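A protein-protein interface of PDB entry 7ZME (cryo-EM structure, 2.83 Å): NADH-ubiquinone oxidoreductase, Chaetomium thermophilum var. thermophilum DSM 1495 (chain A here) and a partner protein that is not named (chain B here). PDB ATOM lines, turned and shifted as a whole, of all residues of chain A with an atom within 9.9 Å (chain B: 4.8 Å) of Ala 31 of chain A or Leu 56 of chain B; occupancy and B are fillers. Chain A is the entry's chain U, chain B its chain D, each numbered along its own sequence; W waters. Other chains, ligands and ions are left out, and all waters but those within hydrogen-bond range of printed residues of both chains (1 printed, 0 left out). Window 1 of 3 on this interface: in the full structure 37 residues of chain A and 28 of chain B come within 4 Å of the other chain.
Water W1 lies within hydrogen-bond range of the side-chain carboxylate (OD1) of Asp 53 of chain B (2.6 Å), the backbone NH (N) of Ser 33 of chain A (3.2 Å) and the guanidinium group (NH1) of Arg 52 of chain B (3.5 Å).
The backbone carbonyl oxygen (O) of Asp 53 of chain B is in hydrogen-bond range of the side-chain hydroxyl (OG1) of Thr 57 of chain B (3.1 Å). The guanidinium group (NH2) of Arg 55 of chain B is in hydrogen-bond range of the backbone carbonyl oxygen (O) of Phe 73 of chain B (2.8 Å). The backbone NH of Asn 66 of chain B sits at hydrogen-bond distance from the side-chain hydroxyl of Thr 64 of chain B (3.3 Å).
Printed residues of chain B within 4 Å of Ala 31 of chain A: Arg 52, Leu 56, Thr 64 and Asn 66. Of the printed residues of chain B, Ser 32 of chain A touches Asp 53 (3.4 Å) and Thr 64 (2.8 Å). Of the printed residues of chain B, Leu 36 of chain A touches Arg 52. Ile 43 of chain A touches none of the printed residues of chain B. Phe 95 of chain A touches none of the printed residues of chain B. Printed residues of chain A within 4 Å of Arg 52 of chain B: Ile 29 (2.9 Å), Ala 31 (3.0 Å) and Leu 36 (3.5 Å). Leu 56 of chain B touches just these residues of chain A: Gly 30 (3.6 Å) and Ala 31 (3.6 Å). No residue of chain A comes within 4 Å of Thr 57 of chain B. Thr 64 of chain B touches four residues of chain A. The nearest residue of chain B that does not touch Ala 31 of chain A is Asp 65 of chain B (4.4 Å).
The backbone carbonyl oxygen of Glu 28 of chain A lies within hydrogen-bond range of the backbone NH of Ala 69 of chain B (3.0 Å). The backbone carbonyl oxygen (O) of Ile 29 of chain A sits at hydrogen-bond distance from the guanidinium group (NH2) of Arg 52 of chain B (2.9 Å). The backbone carbonyl oxygen (O) of Ala 31 of chain A is in hydrogen-bond range of the guanidinium group (NH1) of Arg 52 of chain B (3.0 Å). N of Ala 31 of chain A lies within hydrogen-bond range of O of Asn 66 of chain B (3.2 Å). The side-chain carboxylate (OD1) of Asp 53 of chain B sits close to the side-chain hydroxyl (OG) of Ser 32 of chain A (3.5 Å). The backbone carbonyl oxygen of Thr 64 of chain B lies within hydrogen-bond range of the backbone NH of Ser 32 of chain A, 2.8 Å away. OG of Ser 33 of chain A lies within hydrogen-bond range of OD2 of Asp 53 of chain B (2.8 Å). O of Gly 30 of chain A lies close to O of Asn 66 of chain B (3.3 Å).
Printed residues of chain B that touch a printed residue of chain A: Arg 52, Asp 53, Leu 56, Thr 64, Asp 65, Asn 66, Ala 69 and Phe 73. Hydrophobic or aromatic side chains of chain B within 4 Å of the printed part of chain A: Leu 56, Ala 69 and Phe 73. Printed residues of chain A that touch a printed residue of chain B: Glu 28, Ile 29, Gly 30, Ala 31, Ser 32, Ser 33, Pro 35, Leu 36 and Asn 88. Among the printed residues, 18 pairs touch across the chains.
CB of Glu 28 of chain A touches CD2 of Phe 73 of chain B, 3.8 Å away. Gly 30 of chain A touches Thr 64 of chain B. N of Ala 69 of chain B touches CA of Gly 30 of chain A, 3.6 Å away. O of Ala 31 of chain A touches CD1 of Leu 56 of chain B, at 3.6 Å. Thr 64 of chain B touches Ala 31 of chain A. Thr 64 of chain B touches Pro 35 of chain A (O to CG, 3.4 Å). Arg 52 of chain B touches Leu 36 of chain A. Asn 88 of chain A touches Asp 65 of chain B (ND2 to OD2, 3.7 Å).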
ATOM      1  N   LYS A  27       1.265   7.619  -2.357  1.00  0.00           N
ATOM      2  CA  LYS A  27       0.317   7.011  -1.401  1.00  0.00           C
ATOM      3  C   LYS A  27      -0.827   8.013  -1.221  1.00  0.00           C
ATOM      4  O   LYS A  27      -0.525   9.191  -0.993  1.00  0.00           O
ATOM      5  CB  LYS A  27       1.054   6.675  -0.104  1.00  0.00           C
ATOM      6  CG  LYS A  27       2.339   5.880  -0.280  1.00  0.00           C
ATOM      7  CD  LYS A  27       2.987   5.497   1.032  1.00  0.00           C
ATOM      8  CE  LYS A  27       3.367   6.693   1.877  1.00  0.00           C
ATOM      9  NZ  LYS A  27       4.403   7.524   1.221  1.00  0.00           N
ATOM     10  N   GLU A  28      -2.078   7.554  -1.267  1.00  0.00           N
ATOM     11  CA  GLU A  28      -3.247   8.470  -1.205  1.00  0.00           C
ATOM     12  C   GLU A  28      -3.501   9.007   0.211  1.00  0.00           C
ATOM     13  O   GLU A  28      -2.996   8.414   1.164  1.00  0.00           O
ATOM     14  CB  GLU A  28      -4.476   7.736  -1.739  1.00  0.00           C
ATOM     15  CG  GLU A  28      -4.326   7.185  -3.146  1.00  0.00           C
ATOM     16  CD  GLU A  28      -4.427   8.192  -4.277  1.00  0.00           C
ATOM     17  OE1 GLU A  28      -4.633   9.389  -4.000  1.00  0.00           O
ATOM     18  OE2 GLU A  28      -4.299   7.774  -5.437  1.00  0.00           O
ATOM     19  N   ILE A  29      -4.247  10.108   0.332  1.00  0.00           N
ATOM     20  CA  ILE A  29      -4.625  10.690   1.655  1.00  0.00           C
ATOM     21  C   ILE A  29      -5.587   9.737   2.345  1.00  0.00           C
ATOM     22  O   ILE A  29      -6.536   9.300   1.690  1.00  0.00           O
ATOM     23  CB  ILE A  29      -5.248  12.093   1.483  1.00  0.00           C
ATOM     24  CG1 ILE A  29      -4.249  13.103   0.918  1.00  0.00           C
ATOM     25  CG2 ILE A  29      -5.863  12.583   2.784  1.00  0.00           C
ATOM     26  CD1 ILE A  29      -3.310  13.646   1.947  1.00  0.00           C
ATOM     27  N   GLY A  30      -5.372   9.450   3.611  1.00  0.00           N
ATOM     28  CA  GLY A  30      -6.158   8.526   4.393  1.00  0.00           C
ATOM     29  C   GLY A  30      -7.150   9.145   5.345  1.00  0.00           C
ATOM     30  O   GLY A  30      -7.874   8.412   6.022  1.00  0.00           O
ATOM     31  N   ALA A  31      -7.196  10.468   5.438  1.00  0.00           N
ATOM     32  CA  ALA A  31      -8.126  11.126   6.337  1.00  0.00           C
ATOM     33  C   ALA A  31      -9.539  11.074   5.775  1.00  0.00           C
ATOM     34  O   ALA A  31      -9.748  11.022   4.560  1.00  0.00           O
ATOM     35  CB  ALA A  31      -7.714  12.577   6.575  1.00  0.00           C
ATOM     36  N   SER A  32     -10.513  11.086   6.680  1.00  0.00           N
ATOM     37  CA  SER A  32     -11.921  11.083   6.323  1.00  0.00           C
ATOM     38  C   SER A  32     -12.423  12.520   6.186  1.00  0.00           C
ATOM     39  O   SER A  32     -11.655  13.480   6.277  1.00  0.00           O
ATOM     40  CB  SER A  32     -12.721  10.297   7.355  1.00  0.00           C
ATOM     41  OG  SER A  32     -12.633   8.907   7.119  1.00  0.00           O
ATOM     42  N   SER A  33     -13.730  12.678   5.965  1.00  0.00           N
ATOM     43  CA  SER A  33     -14.291  14.003   5.716  1.00  0.00           C
ATOM     44  C   SER A  33     -14.169  14.908   6.933  1.00  0.00           C
ATOM     45  O   SER A  33     -13.854  16.093   6.798  1.00  0.00           O
ATOM     46  CB  SER A  33     -15.755  13.883   5.286  1.00  0.00           C
ATOM     47  OG  SER A  33     -16.505  13.078   6.176  1.00  0.00           O
ATOM     48  N   ALA A  34     -14.437  14.375   8.131  1.00  0.00           N
ATOM     49  CA  ALA A  34     -14.342  15.206   9.331  1.00  0.00           C
ATOM     50  C   ALA A  34     -12.911  15.632   9.631  1.00  0.00           C
ATOM     51  O   ALA A  34     -12.689  16.831   9.873  1.00  0.00           O
ATOM     52  CB  ALA A  34     -14.997  14.491  10.517  1.00  0.00           C
ATOM     53  N   PRO A  35     -11.907  14.743   9.648  1.00  0.00           N
ATOM     54  CA  PRO A  35     -10.530  15.227   9.832  1.00  0.00           C
ATOM     55  C   PRO A  35     -10.057  16.168   8.741  1.00  0.00           C
ATOM     56  O   PRO A  35      -9.271  17.080   9.024  1.00  0.00           O
ATOM     57  CB  PRO A  35      -9.703  13.935   9.854  1.00  0.00           C
ATOM     58  CG  PRO A  35     -10.646  12.886  10.230  1.00  0.00           C
ATOM     59  CD  PRO A  35     -11.960  13.270   9.654  1.00  0.00           C
ATOM     60  N   LEU A  36     -10.521  15.987   7.501  1.00  0.00           N
ATOM     61  CA  LEU A  36     -10.020  16.843   6.387  1.00  0.00           C
ATOM     62  C   LEU A  36     -10.558  18.270   6.525  1.00  0.00           C
ATOM     63  O   LEU A  36      -9.792  19.190   6.270  1.00  0.00           O
ATOM     64  CB  LEU A  36     -10.338  16.224   5.024  1.00  0.00           C
ATOM     65  CG  LEU A  36      -9.312  15.237   4.477  1.00  0.00           C
ATOM     66  CD1 LEU A  36      -9.746  14.741   3.112  1.00  0.00           C
ATOM     67  CD2 LEU A  36      -7.931  15.861   4.398  1.00  0.00           C
ATOM     68  N   LEU A  37     -11.819  18.440   6.917  1.00  0.00           N
ATOM     69  CA  LEU A  37     -12.430  19.776   7.143  1.00  0.00           C
ATOM     70  C   LEU A  37     -11.787  20.454   8.351  1.00  0.00           C
ATOM     71  O   LEU A  37     -11.637  21.678   8.323  1.00  0.00           O
ATOM     72  CB  LEU A  37     -13.946  19.634   7.290  1.00  0.00           C
ATOM     73  CG  LEU A  37     -14.712  20.871   7.749  1.00  0.00           C
ATOM     74  CD1 LEU A  37     -14.754  21.913   6.649  1.00  0.00           C
ATOM     75  CD2 LEU A  37     -16.120  20.495   8.167  1.00  0.00           C
ATOM     76  N   SER A  38     -11.365  19.686   9.346  1.00  0.00           N
ATOM     77  CA  SER A  38     -10.804  20.274  10.584  1.00  0.00           C
ATOM     78  C   SER A  38      -9.397  20.778  10.280  1.00  0.00           C
ATOM     79  O   SER A  38      -8.952  21.733  10.928  1.00  0.00           O
ATOM     80  CB  SER A  38     -10.748  19.221  11.637  1.00  0.00           C
ATOM     81  OG  SER A  38      -9.855  19.582  12.670  1.00  0.00           O
ATOM     82  N   ALA A  39      -8.751  20.173   9.290  1.00  0.00           N
ATOM     83  CA  ALA A  39      -7.406  20.595   8.928  1.00  0.00           C
ATOM     84  C   ALA A  39      -7.349  21.328   7.594  1.00  0.00           C
ATOM     85  O   ALA A  39      -6.252  21.567   7.083  1.00  0.00           O
ATOM     86  CB  ALA A  39      -6.470  19.389   8.898  1.00  0.00           C
ATOM     87  N   SER A  40      -8.481  21.722   7.026  1.00  0.00           N
ATOM     88  CA  SER A  40      -8.529  22.378   5.693  1.00  0.00           C
ATOM     89  C   SER A  40      -7.812  23.733   5.693  1.00  0.00           C
ATOM     90  O   SER A  40      -7.083  24.017   4.742  1.00  0.00           O
ATOM     91  CB  SER A  40      -9.956  22.525   5.236  1.00  0.00           C
ATOM     92  OG  SER A  40     -10.724  23.206   6.212  1.00  0.00           O
ATOM     93  N   ILE A  43      -4.257  22.932   5.594  1.00  0.00           N
ATOM     94  CA  ILE A  43      -3.873  22.604   4.222  1.00  0.00           C
ATOM     95  C   ILE A  43      -3.476  23.874   3.483  1.00  0.00           C
ATOM     96  O   ILE A  43      -2.342  24.025   3.019  1.00  0.00           O
ATOM     97  CB  ILE A  43      -5.023  21.898   3.483  1.00  0.00           C
ATOM     98  CG1 ILE A  43      -5.448  20.600   4.165  1.00  0.00           C
ATOM     99  CG2 ILE A  43      -4.619  21.616   2.050  1.00  0.00           C
ATOM    100  CD1 ILE A  43      -4.409  19.556   4.181  1.00  0.00           C
ATOM    101  N   THR A  77      -0.742  16.085  -3.028  1.00  0.00           N
ATOM    102  CA  THR A  77      -1.043  14.965  -2.110  1.00  0.00           C
ATOM    103  C   THR A  77       0.043  14.910  -1.045  1.00  0.00           C
ATOM    104  O   THR A  77      -0.304  14.745   0.131  1.00  0.00           O
ATOM    105  CB  THR A  77      -1.051  13.650  -2.897  1.00  0.00           C
ATOM    106  OG1 THR A  77      -1.911  13.806  -4.024  1.00  0.00           O
ATOM    107  CG2 THR A  77      -1.473  12.452  -2.075  1.00  0.00           C
ATOM    108  N   ALA A  80      -0.174  17.673   1.450  1.00  0.00           N
ATOM    109  CA  ALA A  80      -1.294  17.474   2.358  1.00  0.00           C
ATOM    110  C   ALA A  80      -1.050  16.337   3.343  1.00  0.00           C
ATOM    111  O   ALA A  80      -1.582  16.376   4.456  1.00  0.00           O
ATOM    112  CB  ALA A  80      -2.573  17.219   1.563  1.00  0.00           C
ATOM    113  N   ARG A  81      -0.278  15.313   2.966  1.00  0.00           N
ATOM    114  CA  ARG A  81       0.131  14.333   3.964  1.00  0.00           C
ATOM    115  C   ARG A  81       1.105  14.922   4.966  1.00  0.00           C
ATOM    116  O   ARG A  81       1.221  14.399   6.078  1.00  0.00           O
ATOM    117  CB  ARG A  81       0.770  13.091   3.328  1.00  0.00           C
ATOM    118  CG  ARG A  81      -0.186  12.235   2.533  1.00  0.00           C
ATOM    119  CD  ARG A  81       0.463  10.965   1.988  1.00  0.00           C
ATOM    120  NE  ARG A  81       1.457  11.184   0.942  1.00  0.00           N
ATOM    121  CZ  ARG A  81       2.753  10.938   1.086  1.00  0.00           C
ATOM    122  NH1 ARG A  81       3.587  11.156   0.084  1.00  0.00           N
ATOM    123  NH2 ARG A  81       3.215  10.463   2.233  1.00  0.00           N
ATOM    124  N   VAL A  83       1.053  18.065   6.382  1.00  0.00           N
ATOM    125  CA  VAL A  83       0.340  18.747   7.456  1.00  0.00           C
ATOM    126  C   VAL A  83      -0.392  17.744   8.337  1.00  0.00           C
ATOM    127  O   VAL A  83      -0.425  17.888   9.561  1.00  0.00           O
ATOM    128  CB  VAL A  83      -0.618  19.808   6.883  1.00  0.00           C
ATOM    129  CG1 VAL A  83       0.142  20.868   6.132  1.00  0.00           C
ATOM    130  CG2 VAL A  83      -1.595  19.168   5.961  1.00  0.00           C
ATOM    131  N   LEU A  84      -0.979  16.707   7.734  1.00  0.00           N
ATOM    132  CA  LEU A  84      -1.709  15.711   8.512  1.00  0.00           C
ATOM    133  C   LEU A  84      -0.791  15.028   9.513  1.00  0.00           C
ATOM    134  O   LEU A  84      -1.132  14.891  10.692  1.00  0.00           O
ATOM    135  CB  LEU A  84      -2.352  14.684   7.581  1.00  0.00           C
ATOM    136  CG  LEU A  84      -3.676  15.092   6.937  1.00  0.00           C
ATOM    137  CD1 LEU A  84      -3.881  14.375   5.623  1.00  0.00           C
ATOM    138  CD2 LEU A  84      -4.827  14.821   7.874  1.00  0.00           C
ATOM    139  N   LYS A  85       0.391  14.606   9.062  1.00  0.00           N
ATOM    140  CA  LYS A  85       1.367  14.031   9.975  1.00  0.00           C
ATOM    141  C   LYS A  85       1.786  15.042  11.032  1.00  0.00           C
ATOM    142  O   LYS A  85       1.956  14.694  12.206  1.00  0.00           O
ATOM    143  CB  LYS A  85       2.582  13.537   9.195  1.00  0.00           C
ATOM    144  CG  LYS A  85       2.309  12.338   8.313  1.00  0.00           C
ATOM    145  CD  LYS A  85       3.541  11.955   7.515  1.00  0.00           C
ATOM    146  CE  LYS A  85       4.614  11.357   8.412  1.00  0.00           C
ATOM    147  NZ  LYS A  85       4.204  10.037   8.961  1.00  0.00           N
ATOM    148  N   ILE A  87       0.004  17.637  12.195  1.00  0.00           N
ATOM    149  CA  ILE A  87      -1.118  17.739  13.121  1.00  0.00           C
ATOM    150  C   ILE A  87      -1.306  16.471  13.937  1.00  0.00           C
ATOM    151  O   ILE A  87      -2.079  16.468  14.898  1.00  0.00           O
ATOM    152  CB  ILE A  87      -2.396  18.109  12.333  1.00  0.00           C
ATOM    153  CG1 ILE A  87      -2.152  19.362  11.501  1.00  0.00           C
ATOM    154  CG2 ILE A  87      -3.570  18.385  13.250  1.00  0.00           C
ATOM    155  CD1 ILE A  87      -3.260  19.671  10.545  1.00  0.00           C
ATOM    156  N   ASN A  88      -0.621  15.388  13.584  1.00  0.00           N
ATOM    157  CA  ASN A  88      -0.689  14.155  14.357  1.00  0.00           C
ATOM    158  C   ASN A  88       0.481  13.988  15.313  1.00  0.00           C
ATOM    159  O   ASN A  88       0.294  13.480  16.422  1.00  0.00           O
ATOM    160  CB  ASN A  88      -0.760  12.945  13.425  1.00  0.00           C
ATOM    161  CG  ASN A  88      -2.086  12.847  12.705  1.00  0.00           C
ATOM    162  OD1 ASN A  88      -2.143  12.492  11.529  1.00  0.00           O
ATOM    163  ND2 ASN A  88      -3.165  13.165  13.408  1.00  0.00           N
ATOM    164  N   PHE A  95      -6.833  17.975  17.794  1.00  0.00           N
ATOM    165  CA  PHE A  95      -7.310  17.674  16.421  1.00  0.00           C
ATOM    166  C   PHE A  95      -8.487  16.710  16.494  1.00  0.00           C
ATOM    167  O   PHE A  95      -9.511  16.962  15.853  1.00  0.00           O
ATOM    168  CB  PHE A  95      -6.185  17.071  15.584  1.00  0.00           C
ATOM    169  CG  PHE A  95      -6.550  16.730  14.162  1.00  0.00           C
ATOM    170  CD1 PHE A  95      -7.128  17.673  13.330  1.00  0.00           C
ATOM    171  CD2 PHE A  95      -6.292  15.470  13.650  1.00  0.00           C
ATOM    172  CE1 PHE A  95      -7.452  17.361  12.022  1.00  0.00           C
ATOM    173  CE2 PHE A  95      -6.617  15.159  12.341  1.00  0.00           C
ATOM    174  CZ  PHE A  95      -7.196  16.105  11.532  1.00  0.00           C
ATOM    175  N   TRP A  99     -12.511  17.371  15.144  1.00  0.00           N
ATOM    176  CA  TRP A  99     -13.209  16.682  14.064  1.00  0.00           C
ATOM    177  C   TRP A  99     -14.183  15.633  14.578  1.00  0.00           C
ATOM    178  O   TRP A  99     -15.116  15.272  13.855  1.00  0.00           O
ATOM    179  CB  TRP A  99     -12.214  16.071  13.062  1.00  0.00           C
ATOM    180  CG  TRP A  99     -11.369  14.907  13.520  1.00  0.00           C
ATOM    181  CD1 TRP A  99     -10.039  14.934  13.794  1.00  0.00           C
ATOM    182  CD2 TRP A  99     -11.781  13.543  13.689  1.00  0.00           C
ATOM    183  NE1 TRP A  99      -9.598  13.687  14.155  1.00  0.00           N
ATOM    184  CE2 TRP A  99     -10.650  12.815  14.097  1.00  0.00           C
ATOM    185  CE3 TRP A  99     -12.996  12.873  13.550  1.00  0.00           C
ATOM    186  CZ2 TRP A  99     -10.699  11.451  14.369  1.00  0.00           C
ATOM    187  CZ3 TRP A  99     -13.045  11.523  13.823  1.00  0.00           C
ATOM    188  CH2 TRP A  99     -11.903  10.825  14.225  1.00  0.00           C
ATOM    189  N   GLN A 107     -21.024  18.634  10.419  1.00  0.00           N
ATOM    190  CA  GLN A 107     -19.785  19.187   9.808  1.00  0.00           C
ATOM    191  C   GLN A 107     -19.938  20.698   9.632  1.00  0.00           C
ATOM    192  O   GLN A 107     -19.497  21.218   8.603  1.00  0.00           O
ATOM    193  CB  GLN A 107     -19.391  18.389   8.563  1.00  0.00           C
ATOM    194  CG  GLN A 107     -18.916  16.983   8.895  1.00  0.00           C
ATOM    195  CD  GLN A 107     -18.243  16.290   7.736  1.00  0.00           C
ATOM    196  OE1 GLN A 107     -18.011  16.875   6.682  1.00  0.00           O
ATOM    197  NE2 GLN A 107     -17.918  15.024   7.929  1.00  0.00           N
ATOM    198  N   ARG B  52     -16.718   8.544   0.158  1.00  0.00           N
ATOM    199  CA  ARG B  52     -15.255   8.428   0.370  1.00  0.00           C
ATOM    200  C   ARG B  52     -14.981   7.808   1.745  1.00  0.00           C
ATOM    201  O   ARG B  52     -14.001   7.074   1.866  1.00  0.00           O
ATOM    202  CB  ARG B  52     -14.552   9.752   0.057  1.00  0.00           C
ATOM    203  CG  ARG B  52     -13.041   9.615  -0.054  1.00  0.00           C
ATOM    204  CD  ARG B  52     -12.306  10.870  -0.472  1.00  0.00           C
ATOM    205  NE  ARG B  52     -10.876  10.677  -0.296  1.00  0.00           N
ATOM    206  CZ  ARG B  52     -10.198  11.048   0.782  1.00  0.00           C
ATOM    207  NH1 ARG B  52     -10.816  11.660   1.776  1.00  0.00           N
ATOM    208  NH2 ARG B  52      -8.901  10.819   0.858  1.00  0.00           N
ATOM    209  N   ASP B  53     -15.784   8.129   2.751  1.00  0.00           N
ATOM    210  CA  ASP B  53     -15.638   7.552   4.119  1.00  0.00           C
ATOM    211  C   ASP B  53     -15.880   6.036   4.115  1.00  0.00           C
ATOM    212  O   ASP B  53     -15.167   5.338   4.836  1.00  0.00           O
ATOM    213  CB  ASP B  53     -16.587   8.237   5.106  1.00  0.00           C
ATOM    214  CG  ASP B  53     -16.206   9.663   5.444  1.00  0.00           C
ATOM    215  OD1 ASP B  53     -15.125  10.095   5.020  1.00  0.00           O
ATOM    216  OD2 ASP B  53     -17.000  10.327   6.128  1.00  0.00           O
ATOM    217  N   ARG B  54     -16.872   5.555   3.363  1.00  0.00           N
ATOM    218  CA  ARG B  54     -17.138   4.100   3.228  1.00  0.00           C
ATOM    219  C   ARG B  54     -15.919   3.457   2.568  1.00  0.00           C
ATOM    220  O   ARG B  54     -15.581   2.329   2.930  1.00  0.00           O
ATOM    221  CB  ARG B  54     -18.438   3.869   2.455  1.00  0.00           C
ATOM    222  CG  ARG B  54     -18.961   2.443   2.520  1.00  0.00           C
ATOM    223  CD  ARG B  54     -19.670   1.967   1.270  1.00  0.00           C
ATOM    224  NE  ARG B  54     -21.109   2.179   1.252  1.00  0.00           N
ATOM    225  CZ  ARG B  54     -21.742   2.943   0.374  1.00  0.00           C
ATOM    226  NH1 ARG B  54     -23.058   3.061   0.428  1.00  0.00           N
ATOM    227  NH2 ARG B  54     -21.061   3.581  -0.558  1.00  0.00           N
ATOM    228  N   ARG B  55     -15.276   4.164   1.640  1.00  0.00           N
ATOM    229  CA  ARG B  55     -14.053   3.661   0.972  1.00  0.00           C
ATOM    230  C   ARG B  55     -12.940   3.411   1.999  1.00  0.00           C
ATOM    231  O   ARG B  55     -12.155   2.479   1.776  1.00  0.00           O
ATOM    232  CB  ARG B  55     -13.623   4.622  -0.134  1.00  0.00           C
ATOM    233  CG  ARG B  55     -14.492   4.600  -1.379  1.00  0.00           C
ATOM    234  CD  ARG B  55     -13.991   5.664  -2.331  1.00  0.00           C
ATOM    235  NE  ARG B  55     -12.642   5.380  -2.789  1.00  0.00           N
ATOM    236  CZ  ARG B  55     -11.855   6.263  -3.387  1.00  0.00           C
ATOM    237  NH1 ARG B  55     -12.278   7.499  -3.583  1.00  0.00           N
ATOM    238  NH2 ARG B  55     -10.643   5.911  -3.777  1.00  0.00           N
ATOM    239  N   LEU B  56     -12.838   4.226   3.050  1.00  0.00           N
ATOM    240  CA  LEU B  56     -11.741   4.079   4.043  1.00  0.00           C
ATOM    241  C   LEU B  56     -12.181   3.249   5.257  1.00  0.00           C
ATOM    242  O   LEU B  56     -11.322   2.560   5.809  1.00  0.00           O
ATOM    243  CB  LEU B  56     -11.310   5.480   4.485  1.00  0.00           C
ATOM    244  CG  LEU B  56     -10.622   6.349   3.437  1.00  0.00           C
ATOM    245  CD1 LEU B  56     -11.003   7.811   3.604  1.00  0.00           C
ATOM    246  CD2 LEU B  56      -9.114   6.183   3.502  1.00  0.00           C
ATOM    247  N   THR B  57     -13.454   3.284   5.659  1.00  0.00           N
ATOM    248  CA  THR B  57     -13.875   2.602   6.874  1.00  0.00           C
ATOM    249  C   THR B  57     -14.958   1.556   6.668  1.00  0.00           C
ATOM    250  O   THR B  57     -15.159   0.729   7.562  1.00  0.00           O
ATOM    251  CB  THR B  57     -14.384   3.615   7.917  1.00  0.00           C
ATOM    252  OG1 THR B  57     -15.702   4.049   7.563  1.00  0.00           O
ATOM    253  CG2 THR B  57     -13.459   4.823   8.012  1.00  0.00           C
ATOM    254  N   GLY B  58     -15.661   1.570   5.539  1.00  0.00           N
ATOM    255  CA  GLY B  58     -16.749   0.653   5.294  1.00  0.00           C
ATOM    256  C   GLY B  58     -18.112   1.173   5.693  1.00  0.00           C
ATOM    257  O   GLY B  58     -19.123   0.691   5.175  1.00  0.00           O
ATOM    258  N   THR B  64     -11.704   8.326   9.983  1.00  0.00           N
ATOM    259  CA  THR B  64     -10.315   7.917  10.301  1.00  0.00           C
ATOM    260  C   THR B  64      -9.402   9.116  10.032  1.00  0.00           C
ATOM    261  O   THR B  64      -9.615   9.822   9.048  1.00  0.00           O
ATOM    262  CB  THR B  64      -9.852   6.766   9.409  1.00  0.00           C
ATOM    263  OG1 THR B  64      -8.447   6.627   9.615  1.00  0.00           O
ATOM    264  CG2 THR B  64     -10.148   6.966   7.940  1.00  0.00           C
ATOM    265  N   ASP B  65      -8.436   9.345  10.836  1.00  0.00           N
ATOM    266  CA  ASP B  65      -7.483  10.473  10.718  1.00  0.00           C
ATOM    267  C   ASP B  65      -6.139  10.027  10.138  1.00  0.00           C
ATOM    268  O   ASP B  65      -5.257  10.894  10.038  1.00  0.00           O
ATOM    269  CB  ASP B  65      -7.254  11.115  12.089  1.00  0.00           C
ATOM    270  CG  ASP B  65      -6.617  10.219  13.129  1.00  0.00           C
ATOM    271  OD1 ASP B  65      -6.843   8.999  13.075  1.00  0.00           O
ATOM    272  OD2 ASP B  65      -5.899  10.756  13.988  1.00  0.00           O
ATOM    273  N   ASN B  66      -5.971   8.751   9.778  1.00  0.00           N
ATOM    274  CA  ASN B  66      -4.672   8.205   9.314  1.00  0.00           C
ATOM    275  C   ASN B  66      -4.149   8.995   8.113  1.00  0.00           C
ATOM    276  O   ASN B  66      -4.878   9.049   7.149  1.00  0.00           O
ATOM    277  CB  ASN B  66      -4.821   6.739   8.925  1.00  0.00           C
ATOM    278  CG  ASN B  66      -3.529   5.954   9.014  1.00  0.00           C
ATOM    279  OD1 ASN B  66      -2.507   6.354   8.463  1.00  0.00           O
ATOM    280  ND2 ASN B  66      -3.571   4.822   9.698  1.00  0.00           N
ATOM    281  N   ALA B  69      -3.571   6.284   3.240  1.00  0.00           N
ATOM    282  CA  ALA B  69      -4.719   5.445   2.949  1.00  0.00           C
ATOM    283  C   ALA B  69      -4.348   3.967   3.064  1.00  0.00           C
ATOM    284  O   ALA B  69      -3.201   3.587   2.812  1.00  0.00           O
ATOM    285  CB  ALA B  69      -5.252   5.738   1.550  1.00  0.00           C
ATOM    286  N   PRO B  70      -5.327   3.083   3.432  1.00  0.00           N
ATOM    287  CA  PRO B  70      -5.085   1.651   3.464  1.00  0.00           C
ATOM    288  C   PRO B  70      -4.921   1.085   2.049  1.00  0.00           C
ATOM    289  O   PRO B  70      -5.475   1.629   1.134  1.00  0.00           O
ATOM    290  CB  PRO B  70      -6.361   1.077   4.075  1.00  0.00           C
ATOM    291  CG  PRO B  70      -7.428   2.057   3.715  1.00  0.00           C
ATOM    292  CD  PRO B  70      -6.714   3.372   3.881  1.00  0.00           C
ATOM    293  N   PHE B  73      -7.180   1.243  -1.636  1.00  0.00           N
ATOM    294  CA  PHE B  73      -7.990   2.491  -1.665  1.00  0.00           C
ATOM    295  C   PHE B  73      -8.026   3.027  -3.094  1.00  0.00           C
ATOM    296  O   PHE B  73      -9.050   3.574  -3.503  1.00  0.00           O
ATOM    297  CB  PHE B  73      -7.497   3.510  -0.640  1.00  0.00           C
ATOM    298  CG  PHE B  73      -8.298   4.782  -0.576  1.00  0.00           C
ATOM    299  CD1 PHE B  73      -9.560   4.799  -0.008  1.00  0.00           C
ATOM    300  CD2 PHE B  73      -7.788   5.966  -1.082  1.00  0.00           C
ATOM    301  CE1 PHE B  73     -10.297   5.970   0.046  1.00  0.00           C
ATOM    302  CE2 PHE B  73      -8.526   7.135  -1.023  1.00  0.00           C
ATOM    303  CZ  PHE B  73      -9.777   7.134  -0.459  1.00  0.00           C
HETATM  304  O   HOH W   1     -14.051  11.384   3.012  1.00  0.00           O
